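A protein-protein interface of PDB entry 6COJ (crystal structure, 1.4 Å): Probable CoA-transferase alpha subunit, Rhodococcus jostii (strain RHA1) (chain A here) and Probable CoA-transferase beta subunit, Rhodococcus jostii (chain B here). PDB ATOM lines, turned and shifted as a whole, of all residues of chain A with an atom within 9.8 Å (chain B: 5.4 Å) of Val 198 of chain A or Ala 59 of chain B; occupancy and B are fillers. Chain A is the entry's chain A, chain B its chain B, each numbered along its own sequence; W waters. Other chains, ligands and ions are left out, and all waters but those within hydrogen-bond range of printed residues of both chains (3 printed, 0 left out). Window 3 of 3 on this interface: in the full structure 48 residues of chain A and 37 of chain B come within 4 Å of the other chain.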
ATOM      1  N   ARG A  44      -4.887  21.701   5.818  1.00  0.00           N
ATOM      2  CA  ARG A  44      -4.815  22.126   7.216  1.00  0.00           C
ATOM      3  C   ARG A  44      -3.757  23.207   7.362  1.00  0.00           C
ATOM      4  O   ARG A  44      -2.572  22.964   7.099  1.00  0.00           O
ATOM      5  CB  ARG A  44      -4.513  20.948   8.158  1.00  0.00           C
ATOM      6  CG  ARG A  44      -5.384  19.726   7.907  1.00  0.00           C
ATOM      7  CD  ARG A  44      -4.976  18.528   8.756  1.00  0.00           C
ATOM      8  NE  ARG A  44      -5.518  17.287   8.209  1.00  0.00           N
ATOM      9  CZ  ARG A  44      -5.982  16.267   8.921  1.00  0.00           C
ATOM     10  NH1 ARG A  44      -6.019  16.319  10.253  1.00  0.00           N
ATOM     11  NH2 ARG A  44      -6.443  15.193   8.296  1.00  0.00           N
ATOM     12  N   ARG A  45      -4.200  24.385   7.802  1.00  0.00           N
ATOM     13  CA  ARG A  45      -3.355  25.550   8.101  1.00  0.00           C
ATOM     14  C   ARG A  45      -2.288  25.793   7.044  1.00  0.00           C
ATOM     15  O   ARG A  45      -1.113  26.024   7.336  1.00  0.00           O
ATOM     16  CB  ARG A  45      -2.787  25.527   9.521  1.00  0.00           C
ATOM     17  CG  ARG A  45      -2.674  26.943  10.097  1.00  0.00           C
ATOM     18  CD  ARG A  45      -2.129  26.976  11.535  1.00  0.00           C
ATOM     19  NE  ARG A  45      -0.748  26.487  11.549  1.00  0.00           N
ATOM     20  CZ  ARG A  45      -0.292  25.454  12.251  1.00  0.00           C
ATOM     21  NH1 ARG A  45      -1.076  24.790  13.102  1.00  0.00           N
ATOM     22  NH2 ARG A  45       0.984  25.105  12.105  1.00  0.00           N
ATOM     23  N   ASN A 185      -1.368  31.151  14.044  1.00  0.00           N
ATOM     24  CA  ASN A 185      -2.549  31.837  14.545  1.00  0.00           C
ATOM     25  C   ASN A 185      -2.255  33.212  15.125  1.00  0.00           C
ATOM     26  O   ASN A 185      -3.116  34.094  15.080  1.00  0.00           O
ATOM     27  CB  ASN A 185      -3.297  30.964  15.555  1.00  0.00           C
ATOM     28  CG  ASN A 185      -3.773  29.666  14.933  1.00  0.00           C
ATOM     29  OD1 ASN A 185      -4.900  29.582  14.404  1.00  0.00           O
ATOM     30  ND2 ASN A 185      -2.929  28.659  14.972  1.00  0.00           N
ATOM     31  N   TYR A 195       0.897  28.588  17.455  1.00  0.00           N
ATOM     32  CA  TYR A 195      -0.306  27.927  16.988  1.00  0.00           C
ATOM     33  C   TYR A 195      -1.294  27.783  18.140  1.00  0.00           C
ATOM     34  O   TYR A 195      -0.918  27.719  19.316  1.00  0.00           O
ATOM     35  CB  TYR A 195       0.002  26.548  16.394  1.00  0.00           C
ATOM     36  CG  TYR A 195       0.329  25.465  17.407  1.00  0.00           C
ATOM     37  CD1 TYR A 195       1.597  25.372  17.967  1.00  0.00           C
ATOM     38  CD2 TYR A 195      -0.631  24.527  17.791  1.00  0.00           C
ATOM     39  CE1 TYR A 195       1.909  24.365  18.893  1.00  0.00           C
ATOM     40  CE2 TYR A 195      -0.337  23.533  18.714  1.00  0.00           C
ATOM     41  CZ  TYR A 195       0.935  23.454  19.264  1.00  0.00           C
ATOM     42  OH  TYR A 195       1.223  22.446  20.162  1.00  0.00           O
ATOM     43  N   THR A 196      -2.565  27.752  17.782  1.00  0.00           N
ATOM     44  CA  THR A 196      -3.652  27.402  18.674  1.00  0.00           C
ATOM     45  C   THR A 196      -4.381  26.238  18.030  1.00  0.00           C
ATOM     46  O   THR A 196      -4.502  26.164  16.804  1.00  0.00           O
ATOM     47  CB  THR A 196      -4.614  28.583  18.877  1.00  0.00           C
ATOM     48  OG1 THR A 196      -5.173  28.959  17.614  1.00  0.00           O
ATOM     49  CG2 THR A 196      -3.884  29.777  19.465  1.00  0.00           C
ATOM     50  N   GLY A 197      -4.843  25.324  18.847  1.00  0.00           N
ATOM     51  CA  GLY A 197      -5.447  24.113  18.349  1.00  0.00           C
ATOM     52  C   GLY A 197      -4.583  22.910  18.677  1.00  0.00           C
ATOM     53  O   GLY A 197      -3.647  22.972  19.481  1.00  0.00           O
ATOM     54  N   VAL A 198      -4.907  21.795  18.026  1.00  0.00           N
ATOM     55  CA  VAL A 198      -4.377  20.509  18.483  1.00  0.00           C
ATOM     56  C   VAL A 198      -3.051  20.107  17.847  1.00  0.00           C
ATOM     57  O   VAL A 198      -2.461  19.100  18.268  1.00  0.00           O
ATOM     58  CB  VAL A 198      -5.405  19.370  18.330  1.00  0.00           C
ATOM     59  CG1 VAL A 198      -6.653  19.630  19.184  1.00  0.00           C
ATOM     60  CG2 VAL A 198      -5.759  19.158  16.843  1.00  0.00           C
ATOM     61  N   ASP A 199      -2.557  20.834  16.849  1.00  0.00           N
ATOM     62  CA  ASP A 199      -1.377  20.331  16.156  1.00  0.00           C
ATOM     63  C   ASP A 199      -0.529  21.471  15.603  1.00  0.00           C
ATOM     64  O   ASP A 199      -1.026  22.290  14.813  1.00  0.00           O
ATOM     65  CB  ASP A 199      -1.797  19.386  15.023  1.00  0.00           C
ATOM     66  CG  ASP A 199      -0.693  18.419  14.608  1.00  0.00           C
ATOM     67  OD1 ASP A 199       0.497  18.787  14.661  1.00  0.00           O
ATOM     68  OD2 ASP A 199      -1.024  17.279  14.219  1.00  0.00           O
ATOM     69  N   PRO A 200       0.762  21.531  15.946  1.00  0.00           N
ATOM     70  CA  PRO A 200       1.659  22.501  15.291  1.00  0.00           C
ATOM     71  C   PRO A 200       2.013  22.125  13.867  1.00  0.00           C
ATOM     72  O   PRO A 200       2.595  22.952  13.150  1.00  0.00           O
ATOM     73  CB  PRO A 200       2.918  22.447  16.164  1.00  0.00           C
ATOM     74  CG  PRO A 200       2.943  21.033  16.657  1.00  0.00           C
ATOM     75  CD  PRO A 200       1.483  20.676  16.908  1.00  0.00           C
ATOM     76  N   TYR A 201       1.679  20.911  13.432  1.00  0.00           N
ATOM     77  CA  TYR A 201       2.212  20.339  12.188  1.00  0.00           C
ATOM     78  C   TYR A 201       3.736  20.395  12.276  1.00  0.00           C
ATOM     79  O   TYR A 201       4.298  19.919  13.277  1.00  0.00           O
ATOM     80  CB  TYR A 201       1.559  20.940  10.930  1.00  0.00           C
ATOM     81  CG  TYR A 201       0.059  20.873  11.036  1.00  0.00           C
ATOM     82  CD1 TYR A 201      -0.583  19.642  11.208  1.00  0.00           C
ATOM     83  CD2 TYR A 201      -0.717  22.028  11.036  1.00  0.00           C
ATOM     84  CE1 TYR A 201      -1.958  19.567  11.362  1.00  0.00           C
ATOM     85  CE2 TYR A 201      -2.099  21.962  11.182  1.00  0.00           C
ATOM     86  CZ  TYR A 201      -2.714  20.736  11.350  1.00  0.00           C
ATOM     87  OH  TYR A 201      -4.077  20.701  11.518  1.00  0.00           O
ATOM     88  N   ASN A 234       3.267  26.374  22.990  1.00  0.00           N
ATOM     89  CA  ASN A 234       2.688  26.758  21.715  1.00  0.00           C
ATOM     90  C   ASN A 234       3.524  27.798  20.985  1.00  0.00           C
ATOM     91  O   ASN A 234       3.230  28.101  19.824  1.00  0.00           O
ATOM     92  CB  ASN A 234       1.277  27.315  21.955  1.00  0.00           C
ATOM     93  CG  ASN A 234       0.299  26.266  22.467  1.00  0.00           C
ATOM     94  OD1 ASN A 234       0.385  25.831  23.616  1.00  0.00           O
ATOM     95  ND2 ASN A 234      -0.661  25.883  21.627  1.00  0.00           N
ATOM     96  N   LEU A 256      -8.336  24.497   7.115  1.00  0.00           N
ATOM     97  CA  LEU A 256      -8.654  24.777   8.516  1.00  0.00           C
ATOM     98  C   LEU A 256      -7.489  25.496   9.205  1.00  0.00           C
ATOM     99  O   LEU A 256      -6.368  25.551   8.696  1.00  0.00           O
ATOM    100  CB  LEU A 256      -9.070  23.503   9.262  1.00  0.00           C
ATOM    101  CG  LEU A 256      -8.128  22.298   9.344  1.00  0.00           C
ATOM    102  CD1 LEU A 256      -6.951  22.548  10.279  1.00  0.00           C
ATOM    103  CD2 LEU A 256      -8.901  21.059   9.793  1.00  0.00           C
ATOM    104  N   ALA A 257      -7.745  26.030  10.394  1.00  0.00           N
ATOM    105  CA  ALA A 257      -6.706  26.808  11.069  1.00  0.00           C
ATOM    106  C   ALA A 257      -6.822  26.691  12.587  1.00  0.00           C
ATOM    107  O   ALA A 257      -6.946  27.676  13.308  1.00  0.00           O
ATOM    108  CB  ALA A 257      -6.731  28.267  10.623  1.00  0.00           C
ATOM    109  N   GLY A 258      -6.758  25.462  13.089  1.00  0.00           N
ATOM    110  CA  GLY A 258      -6.753  25.262  14.529  1.00  0.00           C
ATOM    111  C   GLY A 258      -7.998  25.853  15.155  1.00  0.00           C
ATOM    112  O   GLY A 258      -9.117  25.642  14.672  1.00  0.00           O
ATOM    113  N   ASP A 259      -7.793  26.627  16.233  1.00  0.00           N
ATOM    114  CA  ASP A 259      -8.891  27.251  16.973  1.00  0.00           C
ATOM    115  C   ASP A 259      -9.541  28.414  16.232  1.00  0.00           C
ATOM    116  O   ASP A 259     -10.626  28.855  16.637  1.00  0.00           O
ATOM    117  CB  ASP A 259      -8.373  27.817  18.300  1.00  0.00           C
ATOM    118  CG  ASP A 259      -8.206  26.761  19.366  1.00  0.00           C
ATOM    119  OD1 ASP A 259      -8.693  25.628  19.171  1.00  0.00           O
ATOM    120  OD2 ASP A 259      -7.588  27.076  20.406  1.00  0.00           O
ATOM    121  N   SER A 260      -8.901  28.949  15.189  1.00  0.00           N
ATOM    122  CA  SER A 260      -9.412  30.159  14.549  1.00  0.00           C
ATOM    123  C   SER A 260     -10.644  29.870  13.704  1.00  0.00           C
ATOM    124  O   SER A 260     -11.623  30.622  13.748  1.00  0.00           O
ATOM    125  CB  SER A 260      -8.321  30.817  13.701  1.00  0.00           C
ATOM    126  OG  SER A 260      -7.234  31.233  14.515  1.00  0.00           O
ATOM    127  N   TYR A 261     -10.600  28.808  12.904  1.00  0.00           N
ATOM    128  CA  TYR A 261     -11.729  28.402  12.078  1.00  0.00           C
ATOM    129  C   TYR A 261     -11.461  27.006  11.540  1.00  0.00           C
ATOM    130  O   TYR A 261     -10.314  26.547  11.484  1.00  0.00           O
ATOM    131  CB  TYR A 261     -12.001  29.384  10.917  1.00  0.00           C
ATOM    132  CG  TYR A 261     -10.759  29.881  10.194  1.00  0.00           C
ATOM    133  CD1 TYR A 261     -10.208  29.169   9.131  1.00  0.00           C
ATOM    134  CD2 TYR A 261     -10.144  31.064  10.571  1.00  0.00           C
ATOM    135  CE1 TYR A 261      -9.074  29.635   8.459  1.00  0.00           C
ATOM    136  CE2 TYR A 261      -9.001  31.530   9.926  1.00  0.00           C
ATOM    137  CZ  TYR A 261      -8.474  30.814   8.870  1.00  0.00           C
ATOM    138  OH  TYR A 261      -7.346  31.278   8.222  1.00  0.00           O
ATOM    139  N   ASP B  56      -8.615  10.002  17.826  1.00  0.00           N
ATOM    140  CA  ASP B  56      -9.701  10.584  17.051  1.00  0.00           C
ATOM    141  C   ASP B  56      -9.350  10.742  15.578  1.00  0.00           C
ATOM    142  O   ASP B  56     -10.103  11.383  14.839  1.00  0.00           O
ATOM    143  CB  ASP B  56     -10.176  11.905  17.676  1.00  0.00           C
ATOM    144  CG  ASP B  56      -9.162  13.037  17.568  1.00  0.00           C
ATOM    145  OD1 ASP B  56      -7.997  12.799  17.171  1.00  0.00           O
ATOM    146  OD2 ASP B  56      -9.537  14.189  17.907  1.00  0.00           O
ATOM    147  N   GLY B  57      -8.236  10.161  15.135  1.00  0.00           N
ATOM    148  CA  GLY B  57      -7.801  10.280  13.761  1.00  0.00           C
ATOM    149  C   GLY B  57      -7.185  11.613  13.425  1.00  0.00           C
ATOM    150  O   GLY B  57      -6.791  11.822  12.267  1.00  0.00           O
ATOM    151  N   GLU B  58      -7.088  12.522  14.398  1.00  0.00           N
ATOM    152  CA  GLU B  58      -6.508  13.842  14.175  1.00  0.00           C
ATOM    153  C   GLU B  58      -5.323  14.079  15.105  1.00  0.00           C
ATOM    154  O   GLU B  58      -4.197  14.225  14.622  1.00  0.00           O
ATOM    155  CB  GLU B  58      -7.542  14.968  14.286  1.00  0.00           C
ATOM    156  CG  GLU B  58      -6.922  16.324  13.995  1.00  0.00           C
ATOM    157  CD  GLU B  58      -7.869  17.517  14.071  1.00  0.00           C
ATOM    158  OE1 GLU B  58      -8.856  17.461  14.837  1.00  0.00           O
ATOM    159  OE2 GLU B  58      -7.602  18.514  13.359  1.00  0.00           O
ATOM    160  N   ALA B  59      -5.534  14.134  16.422  1.00  0.00           N
ATOM    161  CA  ALA B  59      -4.435  14.446  17.333  1.00  0.00           C
ATOM    162  C   ALA B  59      -4.686  14.069  18.789  1.00  0.00           C
ATOM    163  O   ALA B  59      -3.833  14.336  19.638  1.00  0.00           O
ATOM    164  CB  ALA B  59      -4.089  15.938  17.263  1.00  0.00           C
ATOM    165  N   LEU B  60      -5.833  13.476  19.112  1.00  0.00           N
ATOM    166  CA  LEU B  60      -6.186  13.221  20.507  1.00  0.00           C
ATOM    167  C   LEU B  60      -6.263  11.722  20.750  1.00  0.00           C
ATOM    168  O   LEU B  60      -6.866  10.998  19.954  1.00  0.00           O
ATOM    169  CB  LEU B  60      -7.531  13.875  20.854  1.00  0.00           C
ATOM    170  CG  LEU B  60      -7.586  15.394  20.680  1.00  0.00           C
ATOM    171  CD1 LEU B  60      -8.993  15.900  21.009  1.00  0.00           C
ATOM    172  CD2 LEU B  60      -6.542  16.101  21.529  1.00  0.00           C
ATOM    173  N   ILE B  61      -5.653  11.252  21.848  1.00  0.00           N
ATOM    174  CA  ILE B  61      -5.766   9.852  22.253  1.00  0.00           C
ATOM    175  C   ILE B  61      -6.991   9.722  23.149  1.00  0.00           C
ATOM    176  O   ILE B  61      -7.118  10.457  24.133  1.00  0.00           O
ATOM    177  CB  ILE B  61      -4.503   9.384  22.998  1.00  0.00           C
ATOM    178  CG1 ILE B  61      -3.214   9.728  22.238  1.00  0.00           C
ATOM    179  CG2 ILE B  61      -4.585   7.881  23.261  1.00  0.00           C
ATOM    180  CD1 ILE B  61      -1.938   9.300  22.986  1.00  0.00           C
ATOM    181  N   GLY B  76      -4.468  11.582  26.191  1.00  0.00           N
ATOM    182  CA  GLY B  76      -3.139  11.960  25.737  1.00  0.00           C
ATOM    183  C   GLY B  76      -3.191  12.692  24.411  1.00  0.00           C
ATOM    184  O   GLY B  76      -4.263  12.930  23.837  1.00  0.00           O
ATOM    185  N   TRP B  77      -1.996  13.041  23.929  1.00  0.00           N
ATOM    186  CA  TRP B  77      -1.816  13.893  22.759  1.00  0.00           C
ATOM    187  C   TRP B  77      -1.038  13.124  21.701  1.00  0.00           C
ATOM    188  O   TRP B  77      -0.023  12.487  22.009  1.00  0.00           O
ATOM    189  CB  TRP B  77      -1.039  15.145  23.171  1.00  0.00           C
ATOM    190  CG  TRP B  77      -1.014  16.243  22.138  1.00  0.00           C
ATOM    191  CD1 TRP B  77      -2.040  16.642  21.329  1.00  0.00           C
ATOM    192  CD2 TRP B  77       0.100  17.086  21.831  1.00  0.00           C
ATOM    193  NE1 TRP B  77      -1.623  17.686  20.527  1.00  0.00           N
ATOM    194  CE2 TRP B  77      -0.316  17.976  20.815  1.00  0.00           C
ATOM    195  CE3 TRP B  77       1.415  17.169  22.307  1.00  0.00           C
ATOM    196  CZ2 TRP B  77       0.534  18.944  20.273  1.00  0.00           C
ATOM    197  CZ3 TRP B  77       2.261  18.125  21.766  1.00  0.00           C
ATOM    198  CH2 TRP B  77       1.812  19.004  20.755  1.00  0.00           C
ATOM    199  N   MET B  78      -1.501  13.179  20.456  1.00  0.00           N
ATOM    200  CA  MET B  78      -0.877  12.426  19.365  1.00  0.00           C
ATOM    201  C   MET B  78      -0.940  13.240  18.074  1.00  0.00           C
ATOM    202  O   MET B  78      -1.576  12.841  17.092  1.00  0.00           O
ATOM    203  CB  MET B  78      -1.546  11.056  19.234  1.00  0.00           C
ATOM    204  CG  MET B  78      -0.876  10.071  18.278  1.00  0.00           C
ATOM    205  SD  MET B  78       0.876   9.807  18.550  1.00  0.00           S
ATOM    206  CE  MET B  78       0.884   9.222  20.234  1.00  0.00           C
ATOM    207  N   PRO B  79      -0.278  14.397  18.043  1.00  0.00           N
ATOM    208  CA  PRO B  79      -0.164  15.153  16.788  1.00  0.00           C
ATOM    209  C   PRO B  79       0.681  14.383  15.784  1.00  0.00           C
ATOM    210  O   PRO B  79       1.338  13.401  16.115  1.00  0.00           O
ATOM    211  CB  PRO B  79       0.537  16.441  17.230  1.00  0.00           C
ATOM    212  CG  PRO B  79       1.422  15.981  18.367  1.00  0.00           C
ATOM    213  CD  PRO B  79       0.570  14.972  19.110  1.00  0.00           C
HETATM  214  O   HOH W   1      -5.184  18.381  12.213  1.00  0.00           O
HETATM  215  O   HOH W   2      -3.566  16.812  13.710  1.00  0.00           O
HETATM  216  O   HOH W   3      -7.478  14.044  10.796  1.00  0.00           O
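O of Val 198 of chain A lies within hydrogen-bond range of NE1 of Trp 77 of chain B (2.8 Å).
NH1 of Arg 45 of chain A is in hydrogen-bond range of O of Asp 199 of chain A (3.0 Å). O of Pro 200 of chain A sits at hydrogen-bond distance from NH2 of Arg 45 of chain A (2.9 Å). The backbone carbonyl oxygen of Tyr 195 of chain A sits at hydrogen-bond distance from the side-chain amide nitrogen of Asn 234 of chain A, 3.0 Å away. OD1 of Asp 56 of chain B is in hydrogen-bond range of N of Glu 58 of chain B. The backbone NH (N) of Ala 59 of chain B lies within hydrogen-bond range of the side-chain carboxylate (OD1) of Asp 56 of chain B (2.9 Å). N of Met 78 of chain B is in hydrogen-bond range of O of Ala 59 of chain B, at 2.7 Å.
NH1 of Arg 44 of chain A touches CG of Glu 58 of chain B, 3.8 Å away. CH2 of Trp 77 of chain B touches OH of Tyr 195 of chain A, 3.5 Å away. Val 198 of chain A touches Glu 58 of chain B. Val 198 of chain A touches Ala 59 of chain B. Pro 79 of chain B touches Asp 199 of chain A. Trp 77 of chain B touches Pro 200 of chain A.
Printed residues of chain B within 4 Å of Val 198 of chain A: Glu 58, Ala 59 and Trp 77. No residue of chain A comes within 4 Å of Asp 56 of chain B. No residue of chain A comes within 4 Å of Gly 57 of chain B. No residue of chain A comes within 4 Å of Leu 60 of chain B. Printed residues of chain A within 4 Å of Trp 77 of chain B: Tyr 195 (3.5 Å), Val 198 (2.8 Å) and Pro 200 (3.9 Å). Of the printed residues of chain A, Pro 79 of chain B touches Asp 199 (3.4 Å). Of the printed residues of chain B, Asp 199 of chain A touches Pro 79. Of the printed residues of chain B, Arg 44 of chain A touches Glu 58 (3.8 Å). Of the printed residues of chain B, Tyr 195 of chain A touches Trp 77 (3.5 Å). Ile 61 of chain B touches none of the printed residues of chain A. Arg 45 of chain A touches none of the printed residues of chain B. The nearest residue of chain B that does not touch Val 198 of chain A is Pro 79 of chain B (4.1 Å). The nearest printed residue of chain A that does not touch Trp 77 of chain B is Asp 199 of chain A (4.7 Å).
Hydrophobic or aromatic side chains of chain B that line the printed part of chain A: Ala 59, Trp 77 and Pro 79. Of the 17 printed residues of chain A, 5 touch a printed residue of chain B. Hydrophobic or aromatic side chains of chain A that line the printed part of chain B: Tyr 195, Val 198 and Pro 200.
Water W2 bridges OD2 of Asp 199 of chain A and O of Glu 58 of chain B. Water W1 lies within hydrogen-bond range of OH of Tyr 201 of chain A (2.7 Å), OE2 of Glu 58 of chain B (2.7 Å) and NH1 of Arg 44 of chain A (3.0 Å). Water W3 lies within hydrogen-bond range of the backbone carbonyl oxygen of Gly 57 of chain B (2.8 Å) and the guanidinium group of Arg 44 of chain A (2.8 Å).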
